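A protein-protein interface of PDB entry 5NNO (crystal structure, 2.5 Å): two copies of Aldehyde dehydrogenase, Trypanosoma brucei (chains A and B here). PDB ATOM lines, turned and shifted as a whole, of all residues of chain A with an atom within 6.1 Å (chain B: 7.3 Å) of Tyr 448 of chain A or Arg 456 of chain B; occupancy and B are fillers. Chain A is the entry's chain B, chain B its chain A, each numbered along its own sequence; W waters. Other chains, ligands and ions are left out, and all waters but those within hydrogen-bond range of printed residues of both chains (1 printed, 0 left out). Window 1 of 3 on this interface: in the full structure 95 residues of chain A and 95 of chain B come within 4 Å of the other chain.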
ATOM      1  N   SER A 414      -0.747   7.347  30.938  1.00  0.00           N
ATOM      2  CA  SER A 414      -1.999   7.294  31.699  1.00  0.00           C
ATOM      3  C   SER A 414      -2.795   8.572  31.537  1.00  0.00           C
ATOM      4  O   SER A 414      -2.220   9.629  31.237  1.00  0.00           O
ATOM      5  CB  SER A 414      -1.684   7.115  33.183  1.00  0.00           C
ATOM      6  OG  SER A 414      -1.020   8.247  33.751  1.00  0.00           O
ATOM      7  N   GLY A 415      -4.087   8.519  31.828  1.00  0.00           N
ATOM      8  CA  GLY A 415      -4.930   9.733  31.772  1.00  0.00           C
ATOM      9  C   GLY A 415      -4.449  10.924  32.603  1.00  0.00           C
ATOM     10  O   GLY A 415      -4.511  12.044  32.163  1.00  0.00           O
ATOM     11  N   GLY A 430      -8.969  23.653  36.468  1.00  0.00           N
ATOM     12  CA  GLY A 430      -7.932  24.006  35.482  1.00  0.00           C
ATOM     13  C   GLY A 430      -7.123  22.848  34.906  1.00  0.00           C
ATOM     14  O   GLY A 430      -6.113  23.089  34.232  1.00  0.00           O
ATOM     15  N   LEU A 431      -7.543  21.600  35.142  1.00  0.00           N
ATOM     16  CA  LEU A 431      -6.921  20.427  34.476  1.00  0.00           C
ATOM     17  C   LEU A 431      -7.990  19.758  33.627  1.00  0.00           C
ATOM     18  O   LEU A 431      -9.149  19.721  34.038  1.00  0.00           O
ATOM     19  CB  LEU A 431      -6.411  19.377  35.491  1.00  0.00           C
ATOM     20  CG  LEU A 431      -5.345  19.764  36.515  1.00  0.00           C
ATOM     21  CD1 LEU A 431      -4.906  18.510  37.297  1.00  0.00           C
ATOM     22  CD2 LEU A 431      -4.148  20.452  35.872  1.00  0.00           C
ATOM     23  N   PRO A 432      -7.624  19.217  32.451  1.00  0.00           N
ATOM     24  CA  PRO A 432      -8.616  18.392  31.752  1.00  0.00           C
ATOM     25  C   PRO A 432      -8.725  17.021  32.405  1.00  0.00           C
ATOM     26  O   PRO A 432      -7.761  16.531  32.989  1.00  0.00           O
ATOM     27  CB  PRO A 432      -8.077  18.263  30.337  1.00  0.00           C
ATOM     28  CG  PRO A 432      -6.707  18.859  30.344  1.00  0.00           C
ATOM     29  CD  PRO A 432      -6.341  19.248  31.750  1.00  0.00           C
ATOM     30  N   PHE A 433      -9.914  16.427  32.318  1.00  0.00           N
ATOM     31  CA  PHE A 433     -10.180  15.121  32.876  1.00  0.00           C
ATOM     32  C   PHE A 433     -10.574  14.234  31.737  1.00  0.00           C
ATOM     33  O   PHE A 433     -11.519  14.533  31.023  1.00  0.00           O
ATOM     34  CB  PHE A 433     -11.290  15.128  33.943  1.00  0.00           C
ATOM     35  CG  PHE A 433     -11.404  13.815  34.668  1.00  0.00           C
ATOM     36  CD1 PHE A 433     -10.471  13.466  35.632  1.00  0.00           C
ATOM     37  CD2 PHE A 433     -12.416  12.904  34.358  1.00  0.00           C
ATOM     38  CE1 PHE A 433     -10.539  12.242  36.270  1.00  0.00           C
ATOM     39  CE2 PHE A 433     -12.495  11.674  35.000  1.00  0.00           C
ATOM     40  CZ  PHE A 433     -11.549  11.346  35.946  1.00  0.00           C
ATOM     41  N   ALA A 443     -11.316  14.967  26.682  1.00  0.00           N
ATOM     42  CA  ALA A 443     -11.274  15.449  28.032  1.00  0.00           C
ATOM     43  C   ALA A 443     -12.303  16.576  28.229  1.00  0.00           C
ATOM     44  O   ALA A 443     -12.786  17.173  27.278  1.00  0.00           O
ATOM     45  CB  ALA A 443      -9.856  15.916  28.356  1.00  0.00           C
ATOM     46  N   TYR A 444     -12.666  16.816  29.477  1.00  0.00           N
ATOM     47  CA  TYR A 444     -13.633  17.835  29.837  1.00  0.00           C
ATOM     48  C   TYR A 444     -13.374  18.351  31.251  1.00  0.00           C
ATOM     49  O   TYR A 444     -12.354  17.984  31.853  1.00  0.00           O
ATOM     50  CB  TYR A 444     -15.072  17.320  29.589  1.00  0.00           C
ATOM     51  CG  TYR A 444     -15.714  16.406  30.615  1.00  0.00           C
ATOM     52  CD1 TYR A 444     -15.225  15.126  30.860  1.00  0.00           C
ATOM     53  CD2 TYR A 444     -16.890  16.788  31.271  1.00  0.00           C
ATOM     54  CE1 TYR A 444     -15.839  14.291  31.789  1.00  0.00           C
ATOM     55  CE2 TYR A 444     -17.508  15.953  32.195  1.00  0.00           C
ATOM     56  CZ  TYR A 444     -16.979  14.706  32.444  1.00  0.00           C
ATOM     57  OH  TYR A 444     -17.594  13.875  33.360  1.00  0.00           O
ATOM     58  N   HIS A 445     -14.303  19.169  31.754  1.00  0.00           N
ATOM     59  CA  HIS A 445     -14.176  20.061  32.927  1.00  0.00           C
ATOM     60  C   HIS A 445     -13.783  21.482  32.506  1.00  0.00           C
ATOM     61  O   HIS A 445     -12.744  21.670  31.900  1.00  0.00           O
ATOM     62  CB  HIS A 445     -13.224  19.577  34.029  1.00  0.00           C
ATOM     63  CG  HIS A 445     -13.657  18.311  34.705  1.00  0.00           C
ATOM     64  ND1 HIS A 445     -14.643  17.490  34.205  1.00  0.00           N
ATOM     65  CD2 HIS A 445     -13.197  17.708  35.827  1.00  0.00           C
ATOM     66  CE1 HIS A 445     -14.781  16.443  34.998  1.00  0.00           C
ATOM     67  NE2 HIS A 445     -13.920  16.553  35.996  1.00  0.00           N
ATOM     68  N   GLY A 446     -14.644  22.462  32.815  1.00  0.00           N
ATOM     69  CA  GLY A 446     -14.291  23.880  32.796  1.00  0.00           C
ATOM     70  C   GLY A 446     -14.039  24.387  31.377  1.00  0.00           C
ATOM     71  O   GLY A 446     -14.848  24.157  30.496  1.00  0.00           O
ATOM     72  N   ARG A 447     -12.889  25.025  31.153  1.00  0.00           N
ATOM     73  CA  ARG A 447     -12.428  25.356  29.813  1.00  0.00           C
ATOM     74  C   ARG A 447     -12.427  24.178  28.815  1.00  0.00           C
ATOM     75  O   ARG A 447     -12.634  24.379  27.596  1.00  0.00           O
ATOM     76  CB  ARG A 447     -11.018  25.979  29.847  1.00  0.00           C
ATOM     77  CG  ARG A 447     -10.610  26.629  28.509  1.00  0.00           C
ATOM     78  CD  ARG A 447      -9.411  27.583  28.592  1.00  0.00           C
ATOM     79  NE  ARG A 447      -9.590  28.779  27.759  1.00  0.00           N
ATOM     80  CZ  ARG A 447      -9.129  30.012  28.041  1.00  0.00           C
ATOM     81  NH1 ARG A 447      -8.441  30.281  29.166  1.00  0.00           N
ATOM     82  NH2 ARG A 447      -9.354  31.009  27.170  1.00  0.00           N
ATOM     83  N   TYR A 448     -12.170  22.979  29.311  1.00  0.00           N
ATOM     84  CA  TYR A 448     -11.951  21.798  28.457  1.00  0.00           C
ATOM     85  C   TYR A 448     -13.264  21.128  28.052  1.00  0.00           C
ATOM     86  O   TYR A 448     -13.338  20.462  27.022  1.00  0.00           O
ATOM     87  CB  TYR A 448     -11.010  20.791  29.170  1.00  0.00           C
ATOM     88  CG  TYR A 448      -9.715  21.426  29.635  1.00  0.00           C
ATOM     89  CD1 TYR A 448      -8.712  21.769  28.717  1.00  0.00           C
ATOM     90  CD2 TYR A 448      -9.512  21.737  30.975  1.00  0.00           C
ATOM     91  CE1 TYR A 448      -7.550  22.398  29.125  1.00  0.00           C
ATOM     92  CE2 TYR A 448      -8.345  22.357  31.391  1.00  0.00           C
ATOM     93  CZ  TYR A 448      -7.363  22.682  30.474  1.00  0.00           C
ATOM     94  OH  TYR A 448      -6.188  23.296  30.918  1.00  0.00           O
ATOM     95  N   SER A 449     -14.299  21.292  28.867  1.00  0.00           N
ATOM     96  CA  SER A 449     -15.636  20.954  28.424  1.00  0.00           C
ATOM     97  C   SER A 449     -16.095  21.942  27.357  1.00  0.00           C
ATOM     98  O   SER A 449     -16.617  21.501  26.346  1.00  0.00           O
ATOM     99  CB  SER A 449     -16.620  20.949  29.557  1.00  0.00           C
ATOM    100  OG  SER A 449     -16.389  22.087  30.321  1.00  0.00           O
ATOM    101  N   PHE A 450     -15.884  23.246  27.568  1.00  0.00           N
ATOM    102  CA  PHE A 450     -16.244  24.273  26.562  1.00  0.00           C
ATOM    103  C   PHE A 450     -15.499  24.038  25.265  1.00  0.00           C
ATOM    104  O   PHE A 450     -16.088  24.163  24.195  1.00  0.00           O
ATOM    105  CB  PHE A 450     -15.993  25.708  27.085  1.00  0.00           C
ATOM    106  CG  PHE A 450     -16.371  26.824  26.096  1.00  0.00           C
ATOM    107  CD1 PHE A 450     -15.476  27.260  25.123  1.00  0.00           C
ATOM    108  CD2 PHE A 450     -17.600  27.465  26.176  1.00  0.00           C
ATOM    109  CE1 PHE A 450     -15.818  28.273  24.225  1.00  0.00           C
ATOM    110  CE2 PHE A 450     -17.952  28.475  25.293  1.00  0.00           C
ATOM    111  CZ  PHE A 450     -17.063  28.877  24.308  1.00  0.00           C
ATOM    112  N   GLU A 451     -14.206  23.713  25.340  1.00  0.00           N
ATOM    113  CA  GLU A 451     -13.413  23.421  24.111  1.00  0.00           C
ATOM    114  C   GLU A 451     -13.874  22.129  23.410  1.00  0.00           C
ATOM    115  O   GLU A 451     -13.987  22.093  22.193  1.00  0.00           O
ATOM    116  CB  GLU A 451     -11.889  23.483  24.385  1.00  0.00           C
ATOM    117  CG  GLU A 451     -11.403  24.931  24.576  1.00  0.00           C
ATOM    118  CD  GLU A 451      -9.900  25.088  24.727  1.00  0.00           C
ATOM    119  OE1 GLU A 451      -9.460  26.071  25.362  1.00  0.00           O
ATOM    120  OE2 GLU A 451      -9.151  24.243  24.205  1.00  0.00           O
ATOM    121  N   THR A 452     -14.196  21.104  24.186  1.00  0.00           N
ATOM    122  CA  THR A 452     -14.738  19.806  23.679  1.00  0.00           C
ATOM    123  C   THR A 452     -16.084  19.946  22.975  1.00  0.00           C
ATOM    124  O   THR A 452     -16.317  19.304  21.966  1.00  0.00           O
ATOM    125  CB  THR A 452     -14.865  18.762  24.839  1.00  0.00           C
ATOM    126  OG1 THR A 452     -13.554  18.401  25.280  1.00  0.00           O
ATOM    127  CG2 THR A 452     -15.600  17.460  24.408  1.00  0.00           C
ATOM    128  N   PHE A 453     -16.965  20.784  23.510  1.00  0.00           N
ATOM    129  CA  PHE A 453     -18.301  20.986  22.952  1.00  0.00           C
ATOM    130  C   PHE A 453     -18.377  22.197  21.978  1.00  0.00           C
ATOM    131  O   PHE A 453     -19.449  22.778  21.776  1.00  0.00           O
ATOM    132  CB  PHE A 453     -19.329  21.068  24.102  1.00  0.00           C
ATOM    133  CG  PHE A 453     -19.456  19.779  24.907  1.00  0.00           C
ATOM    134  CD1 PHE A 453     -19.890  18.608  24.304  1.00  0.00           C
ATOM    135  CD2 PHE A 453     -19.169  19.741  26.265  1.00  0.00           C
ATOM    136  CE1 PHE A 453     -20.026  17.428  25.038  1.00  0.00           C
ATOM    137  CE2 PHE A 453     -19.290  18.561  26.989  1.00  0.00           C
ATOM    138  CZ  PHE A 453     -19.713  17.402  26.371  1.00  0.00           C
ATOM    139  N   VAL B  98       3.119  22.620  29.954  1.00  0.00           N
ATOM    140  CA  VAL B  98       2.390  23.879  30.139  1.00  0.00           C
ATOM    141  C   VAL B  98       1.831  23.950  31.565  1.00  0.00           C
ATOM    142  O   VAL B  98       1.298  22.973  32.096  1.00  0.00           O
ATOM    143  CB  VAL B  98       1.273  24.039  29.087  1.00  0.00           C
ATOM    144  CG1 VAL B  98       0.507  25.351  29.278  1.00  0.00           C
ATOM    145  CG2 VAL B  98       1.886  24.013  27.690  1.00  0.00           C
ATOM    146  N   LYS B  99       2.001  25.117  32.174  1.00  0.00           N
ATOM    147  CA  LYS B  99       1.498  25.407  33.510  1.00  0.00           C
ATOM    148  C   LYS B  99       0.073  25.950  33.339  1.00  0.00           C
ATOM    149  O   LYS B  99      -0.095  27.114  32.938  1.00  0.00           O
ATOM    150  CB  LYS B  99       2.389  26.459  34.187  1.00  0.00           C
ATOM    151  CG  LYS B  99       3.865  26.078  34.279  1.00  0.00           C
ATOM    152  CD  LYS B  99       4.120  24.946  35.261  1.00  0.00           C
ATOM    153  CE  LYS B  99       4.068  25.437  36.707  1.00  0.00           C
ATOM    154  NZ  LYS B  99       3.671  24.389  37.687  1.00  0.00           N
ATOM    155  N   PRO B 100      -0.954  25.119  33.598  1.00  0.00           N
ATOM    156  CA  PRO B 100      -2.305  25.630  33.408  1.00  0.00           C
ATOM    157  C   PRO B 100      -2.611  26.675  34.468  1.00  0.00           C
ATOM    158  O   PRO B 100      -1.950  26.689  35.489  1.00  0.00           O
ATOM    159  CB  PRO B 100      -3.169  24.389  33.617  1.00  0.00           C
ATOM    160  CG  PRO B 100      -2.411  23.589  34.616  1.00  0.00           C
ATOM    161  CD  PRO B 100      -0.963  23.814  34.289  1.00  0.00           C
ATOM    162  N   THR B 101      -3.597  27.536  34.242  1.00  0.00           N
ATOM    163  CA  THR B 101      -4.083  28.416  35.303  1.00  0.00           C
ATOM    164  C   THR B 101      -5.046  27.624  36.209  1.00  0.00           C
ATOM    165  O   THR B 101      -6.091  27.118  35.766  1.00  0.00           O
ATOM    166  CB  THR B 101      -4.750  29.688  34.752  1.00  0.00           C
ATOM    167  OG1 THR B 101      -3.766  30.471  34.085  1.00  0.00           O
ATOM    168  CG2 THR B 101      -5.344  30.551  35.884  1.00  0.00           C
ATOM    169  N   MET B 102      -4.668  27.532  37.476  1.00  0.00           N
ATOM    170  CA  MET B 102      -5.422  26.782  38.456  1.00  0.00           C
ATOM    171  C   MET B 102      -6.331  27.711  39.251  1.00  0.00           C
ATOM    172  O   MET B 102      -6.037  28.887  39.419  1.00  0.00           O
ATOM    173  CB  MET B 102      -4.466  26.003  39.378  1.00  0.00           C
ATOM    174  CG  MET B 102      -3.580  24.985  38.653  1.00  0.00           C
ATOM    175  SD  MET B 102      -4.407  23.644  37.747  1.00  0.00           S
ATOM    176  CE  MET B 102      -5.271  22.796  39.081  1.00  0.00           C
ATOM    177  N   GLU B 112       0.685  20.601  36.100  1.00  0.00           N
ATOM    178  CA  GLU B 112       1.386  20.584  34.818  1.00  0.00           C
ATOM    179  C   GLU B 112       0.650  19.771  33.738  1.00  0.00           C
ATOM    180  O   GLU B 112       0.056  18.722  34.019  1.00  0.00           O
ATOM    181  CB  GLU B 112       2.777  19.989  35.024  1.00  0.00           C
ATOM    182  CG  GLU B 112       3.917  20.745  34.381  1.00  0.00           C
ATOM    183  CD  GLU B 112       5.245  20.005  34.527  1.00  0.00           C
ATOM    184  OE1 GLU B 112       5.286  18.796  34.206  1.00  0.00           O
ATOM    185  OE2 GLU B 112       6.246  20.632  34.944  1.00  0.00           O
ATOM    186  N   LEU B 113       0.721  20.274  32.494  1.00  0.00           N
ATOM    187  CA  LEU B 113       0.221  19.568  31.314  1.00  0.00           C
ATOM    188  C   LEU B 113       1.405  19.124  30.450  1.00  0.00           C
ATOM    189  O   LEU B 113       2.052  19.948  29.805  1.00  0.00           O
ATOM    190  CB  LEU B 113      -0.694  20.478  30.498  1.00  0.00           C
ATOM    191  CG  LEU B 113      -2.131  20.751  30.954  1.00  0.00           C
ATOM    192  CD1 LEU B 113      -2.272  20.752  32.466  1.00  0.00           C
ATOM    193  CD2 LEU B 113      -2.650  22.058  30.335  1.00  0.00           C
ATOM    194  N   GLN B 114       1.692  17.824  30.438  1.00  0.00           N
ATOM    195  CA  GLN B 114       2.818  17.263  29.660  1.00  0.00           C
ATOM    196  C   GLN B 114       2.269  16.635  28.385  1.00  0.00           C
ATOM    197  O   GLN B 114       1.108  16.246  28.335  1.00  0.00           O
ATOM    198  CB  GLN B 114       3.598  16.226  30.505  1.00  0.00           C
ATOM    199  CG  GLN B 114       3.980  16.705  31.911  1.00  0.00           C
ATOM    200  CD  GLN B 114       4.868  15.730  32.703  1.00  0.00           C
ATOM    201  OE1 GLN B 114       5.118  14.582  32.296  1.00  0.00           O
ATOM    202  NE2 GLN B 114       5.325  16.180  33.875  1.00  0.00           N
ATOM    203  N   TYR B 115       3.085  16.588  27.335  1.00  0.00           N
ATOM    204  CA  TYR B 115       2.696  15.954  26.071  1.00  0.00           C
ATOM    205  C   TYR B 115       3.565  14.732  25.865  1.00  0.00           C
ATOM    206  O   TYR B 115       4.802  14.802  26.009  1.00  0.00           O
ATOM    207  CB  TYR B 115       2.847  16.889  24.868  1.00  0.00           C
ATOM    208  CG  TYR B 115       1.842  18.006  24.825  1.00  0.00           C
ATOM    209  CD1 TYR B 115       0.523  17.770  24.499  1.00  0.00           C
ATOM    210  CD2 TYR B 115       2.226  19.325  25.117  1.00  0.00           C
ATOM    211  CE1 TYR B 115      -0.397  18.814  24.466  1.00  0.00           C
ATOM    212  CE2 TYR B 115       1.316  20.374  25.089  1.00  0.00           C
ATOM    213  CZ  TYR B 115       0.011  20.123  24.763  1.00  0.00           C
ATOM    214  OH  TYR B 115      -0.849  21.214  24.733  1.00  0.00           O
ATOM    215  N   GLU B 116       2.898  13.622  25.530  1.00  0.00           N
ATOM    216  CA  GLU B 116       3.538  12.320  25.402  1.00  0.00           C
ATOM    217  C   GLU B 116       3.011  11.713  24.140  1.00  0.00           C
ATOM    218  O   GLU B 116       1.861  11.969  23.806  1.00  0.00           O
ATOM    219  CB  GLU B 116       3.227  11.400  26.612  1.00  0.00           C
ATOM    220  CG  GLU B 116       1.769  11.006  26.790  1.00  0.00           C
ATOM    221  CD  GLU B 116       1.528   9.940  27.856  1.00  0.00           C
ATOM    222  OE1 GLU B 116       2.340   9.786  28.826  1.00  0.00           O
ATOM    223  OE2 GLU B 116       0.474   9.263  27.728  1.00  0.00           O
ATOM    224  N   LEU B 118       1.499   8.826  21.466  1.00  0.00           N
ATOM    225  CA  LEU B 118       0.367   7.902  21.555  1.00  0.00           C
ATOM    226  C   LEU B 118       0.749   6.482  21.199  1.00  0.00           C
ATOM    227  O   LEU B 118       0.341   5.549  21.891  1.00  0.00           O
ATOM    228  CB  LEU B 118      -0.787   8.349  20.675  1.00  0.00           C
ATOM    229  CG  LEU B 118      -1.590   9.570  21.179  1.00  0.00           C
ATOM    230  CD1 LEU B 118      -2.503  10.085  20.094  1.00  0.00           C
ATOM    231  CD2 LEU B 118      -2.420   9.215  22.413  1.00  0.00           C
ATOM    232  N   GLU B 451      -0.267  18.500  18.312  1.00  0.00           N
ATOM    233  CA  GLU B 451      -1.321  18.375  19.350  1.00  0.00           C
ATOM    234  C   GLU B 451      -2.256  17.169  19.090  1.00  0.00           C
ATOM    235  O   GLU B 451      -2.592  16.419  20.012  1.00  0.00           O
ATOM    236  CB  GLU B 451      -2.097  19.704  19.542  1.00  0.00           C
ATOM    237  CG  GLU B 451      -1.289  20.771  20.300  1.00  0.00           C
ATOM    238  CD  GLU B 451      -2.037  22.091  20.592  1.00  0.00           C
ATOM    239  OE1 GLU B 451      -2.034  23.006  19.759  1.00  0.00           O
ATOM    240  OE2 GLU B 451      -2.616  22.295  21.676  1.00  0.00           O
ATOM    241  N   SER B 454      -0.703  13.588  19.930  1.00  0.00           N
ATOM    242  CA  SER B 454      -0.182  13.603  21.301  1.00  0.00           C
ATOM    243  C   SER B 454      -1.315  13.478  22.324  1.00  0.00           C
ATOM    244  O   SER B 454      -2.443  13.904  22.081  1.00  0.00           O
ATOM    245  CB  SER B 454       0.581  14.898  21.594  1.00  0.00           C
ATOM    246  OG  SER B 454       1.831  14.932  20.928  1.00  0.00           O
ATOM    247  N   HIS B 455      -0.979  12.885  23.462  1.00  0.00           N
ATOM    248  CA  HIS B 455      -1.845  12.836  24.618  1.00  0.00           C
ATOM    249  C   HIS B 455      -1.362  13.925  25.538  1.00  0.00           C
ATOM    250  O   HIS B 455      -0.215  13.904  25.994  1.00  0.00           O
ATOM    251  CB  HIS B 455      -1.763  11.478  25.317  1.00  0.00           C
ATOM    252  CG  HIS B 455      -2.423  11.452  26.657  1.00  0.00           C
ATOM    253  ND1 HIS B 455      -3.762  11.704  26.827  1.00  0.00           N
ATOM    254  CD2 HIS B 455      -1.918  11.241  27.896  1.00  0.00           C
ATOM    255  CE1 HIS B 455      -4.056  11.633  28.115  1.00  0.00           C
ATOM    256  NE2 HIS B 455      -2.955  11.343  28.783  1.00  0.00           N
ATOM    257  N   ARG B 456      -2.244  14.898  25.775  1.00  0.00           N
ATOM    258  CA  ARG B 456      -2.030  15.899  26.801  1.00  0.00           C
ATOM    259  C   ARG B 456      -2.319  15.241  28.181  1.00  0.00           C
ATOM    260  O   ARG B 456      -3.464  14.871  28.468  1.00  0.00           O
ATOM    261  CB  ARG B 456      -2.931  17.091  26.558  1.00  0.00           C
ATOM    262  CG  ARG B 456      -2.628  18.221  27.526  1.00  0.00           C
ATOM    263  CD  ARG B 456      -3.415  19.469  27.208  1.00  0.00           C
ATOM    264  NE  ARG B 456      -4.838  19.207  27.285  1.00  0.00           N
ATOM    265  CZ  ARG B 456      -5.787  20.018  26.826  1.00  0.00           C
ATOM    266  NH1 ARG B 456      -5.482  21.167  26.226  1.00  0.00           N
ATOM    267  NH2 ARG B 456      -7.067  19.651  26.971  1.00  0.00           N
ATOM    268  N   ARG B 457      -1.273  15.098  28.996  1.00  0.00           N
ATOM    269  CA  ARG B 457      -1.338  14.369  30.277  1.00  0.00           C
ATOM    270  C   ARG B 457      -1.231  15.343  31.464  1.00  0.00           C
ATOM    271  O   ARG B 457      -0.181  15.950  31.676  1.00  0.00           O
ATOM    272  CB  ARG B 457      -0.219  13.340  30.348  1.00  0.00           C
ATOM    273  CG  ARG B 457      -0.378  12.272  31.422  1.00  0.00           C
ATOM    274  CD  ARG B 457       0.976  11.652  31.723  1.00  0.00           C
ATOM    275  NE  ARG B 457       0.884  10.374  32.433  1.00  0.00           N
ATOM    276  CZ  ARG B 457       1.843   9.448  32.489  1.00  0.00           C
ATOM    277  NH1 ARG B 457       3.011   9.633  31.893  1.00  0.00           N
ATOM    278  NH2 ARG B 457       1.621   8.329  33.173  1.00  0.00           N
ATOM    279  N   PRO B 458      -2.323  15.522  32.215  1.00  0.00           N
ATOM    280  CA  PRO B 458      -2.245  16.239  33.483  1.00  0.00           C
ATOM    281  C   PRO B 458      -1.428  15.512  34.582  1.00  0.00           C
ATOM    282  O   PRO B 458      -1.511  14.286  34.744  1.00  0.00           O
ATOM    283  CB  PRO B 458      -3.714  16.371  33.917  1.00  0.00           C
ATOM    284  CG  PRO B 458      -4.448  15.337  33.122  1.00  0.00           C
ATOM    285  CD  PRO B 458      -3.721  15.284  31.823  1.00  0.00           C
HETATM  286  O   HOH W   1      -9.262  21.107  24.961  1.00  0.00           O
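The backbone NH of Leu 113 of chain B is in hydrogen-bond range of the backbone carbonyl oxygen of Val 98 of chain B, 2.8 Å away.
O of Gln 114 of chain B is in hydrogen-bond range of N of Arg 457 of chain B (2.7 Å).
The backbone carbonyl oxygen (O) of Glu 116 of chain B is in hydrogen-bond range of the backbone NH (N) of His 455 of chain B (3.0 Å).
The guanidinium group (NH1) of Arg 457 of chain B lies within salt-bridge range of the side-chain carboxylate (OE1) of Glu 116 of chain B (3.1 Å).
The backbone carbonyl oxygen (O) of Gly 430 of chain A lies within hydrogen-bond range of the side-chain hydroxyl (OH) of Tyr 448 of chain A (3.3 Å).
The backbone carbonyl oxygen (O) of Tyr 448 of chain A lies within hydrogen-bond range of the side-chain hydroxyl (OG1) of Thr 452 of chain A.
Water W1 bridges OE2 of Glu 451 of chain A and NH2 of Arg 456 of chain B.
Among the printed residues, merely in contact across the chains: Ser 414 of chain A with Glu 116 of chain B (3.9 Å), Gly 415 of chain A with His 455 of chain B (3.8 Å), Gly 415 of chain A with Pro 458 of chain B (3.4 Å), Gly 430 of chain A with Pro 100 of chain B (3.3 Å), Gly 430 of chain A with Thr 101 of chain B (3.6 Å), Gly 430 of chain A with Met 102 of chain B (3.9 Å), Leu 431 of chain A with Pro 100 of chain B (3.8 Å), Leu 431 of chain A with Met 102 of chain B (3.7 Å), Leu 431 of chain A with Leu 113 of chain B (3.9 Å), Pro 432 of chain A with Arg 456 of chain B (3.5 Å), Pro 432 of chain A with Pro 458 of chain B (3.5 Å), Tyr 448 of chain A with Leu 113 of chain B (3.8 Å) and Tyr 448 of chain A with Arg 456 of chain B (3.2 Å).
Among the printed residues, no Asp or Glu carboxylate lies within 4 Å of a Lys or Arg side-chain nitrogen of the other chain.
Position printed for both chains: 451.
A ring nitrogen (NE2) of His 455 of chain B lies within hydrogen-bond range of the backbone carbonyl oxygen (O) of Ser 414 of chain A.
NH2 of Arg 457 of chain B lies within hydrogen-bond range of OG of Ser 414 of chain A (2.7 Å).
Of the printed residues of chain B, Leu 431 of chain A touches Pro 100 (3.8 Å), Met 102 (3.7 Å) and Leu 113 (3.9 Å).
Of the printed residues of chain B, Pro 432 of chain A touches Arg 456 (3.5 Å) and Pro 458 (3.5 Å).
Tyr 448 of chain A touches just these residues of chain B: Leu 113 (3.8 Å) and Arg 456 (3.2 Å).
Of the printed residues of chain A, Glu 116 of chain B touches Ser 414.
Arg 456 of chain B touches just these residues of chain A: Pro 432 (3.5 Å) and Tyr 448 (3.2 Å).
The nearest residue of chain A that does not touch Arg 456 of chain B is Gly 415 of chain A (4.8 Å).
The nearest printed residue of chain A that does not touch Pro 100 of chain B is Tyr 448 of chain A (4.2 Å).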
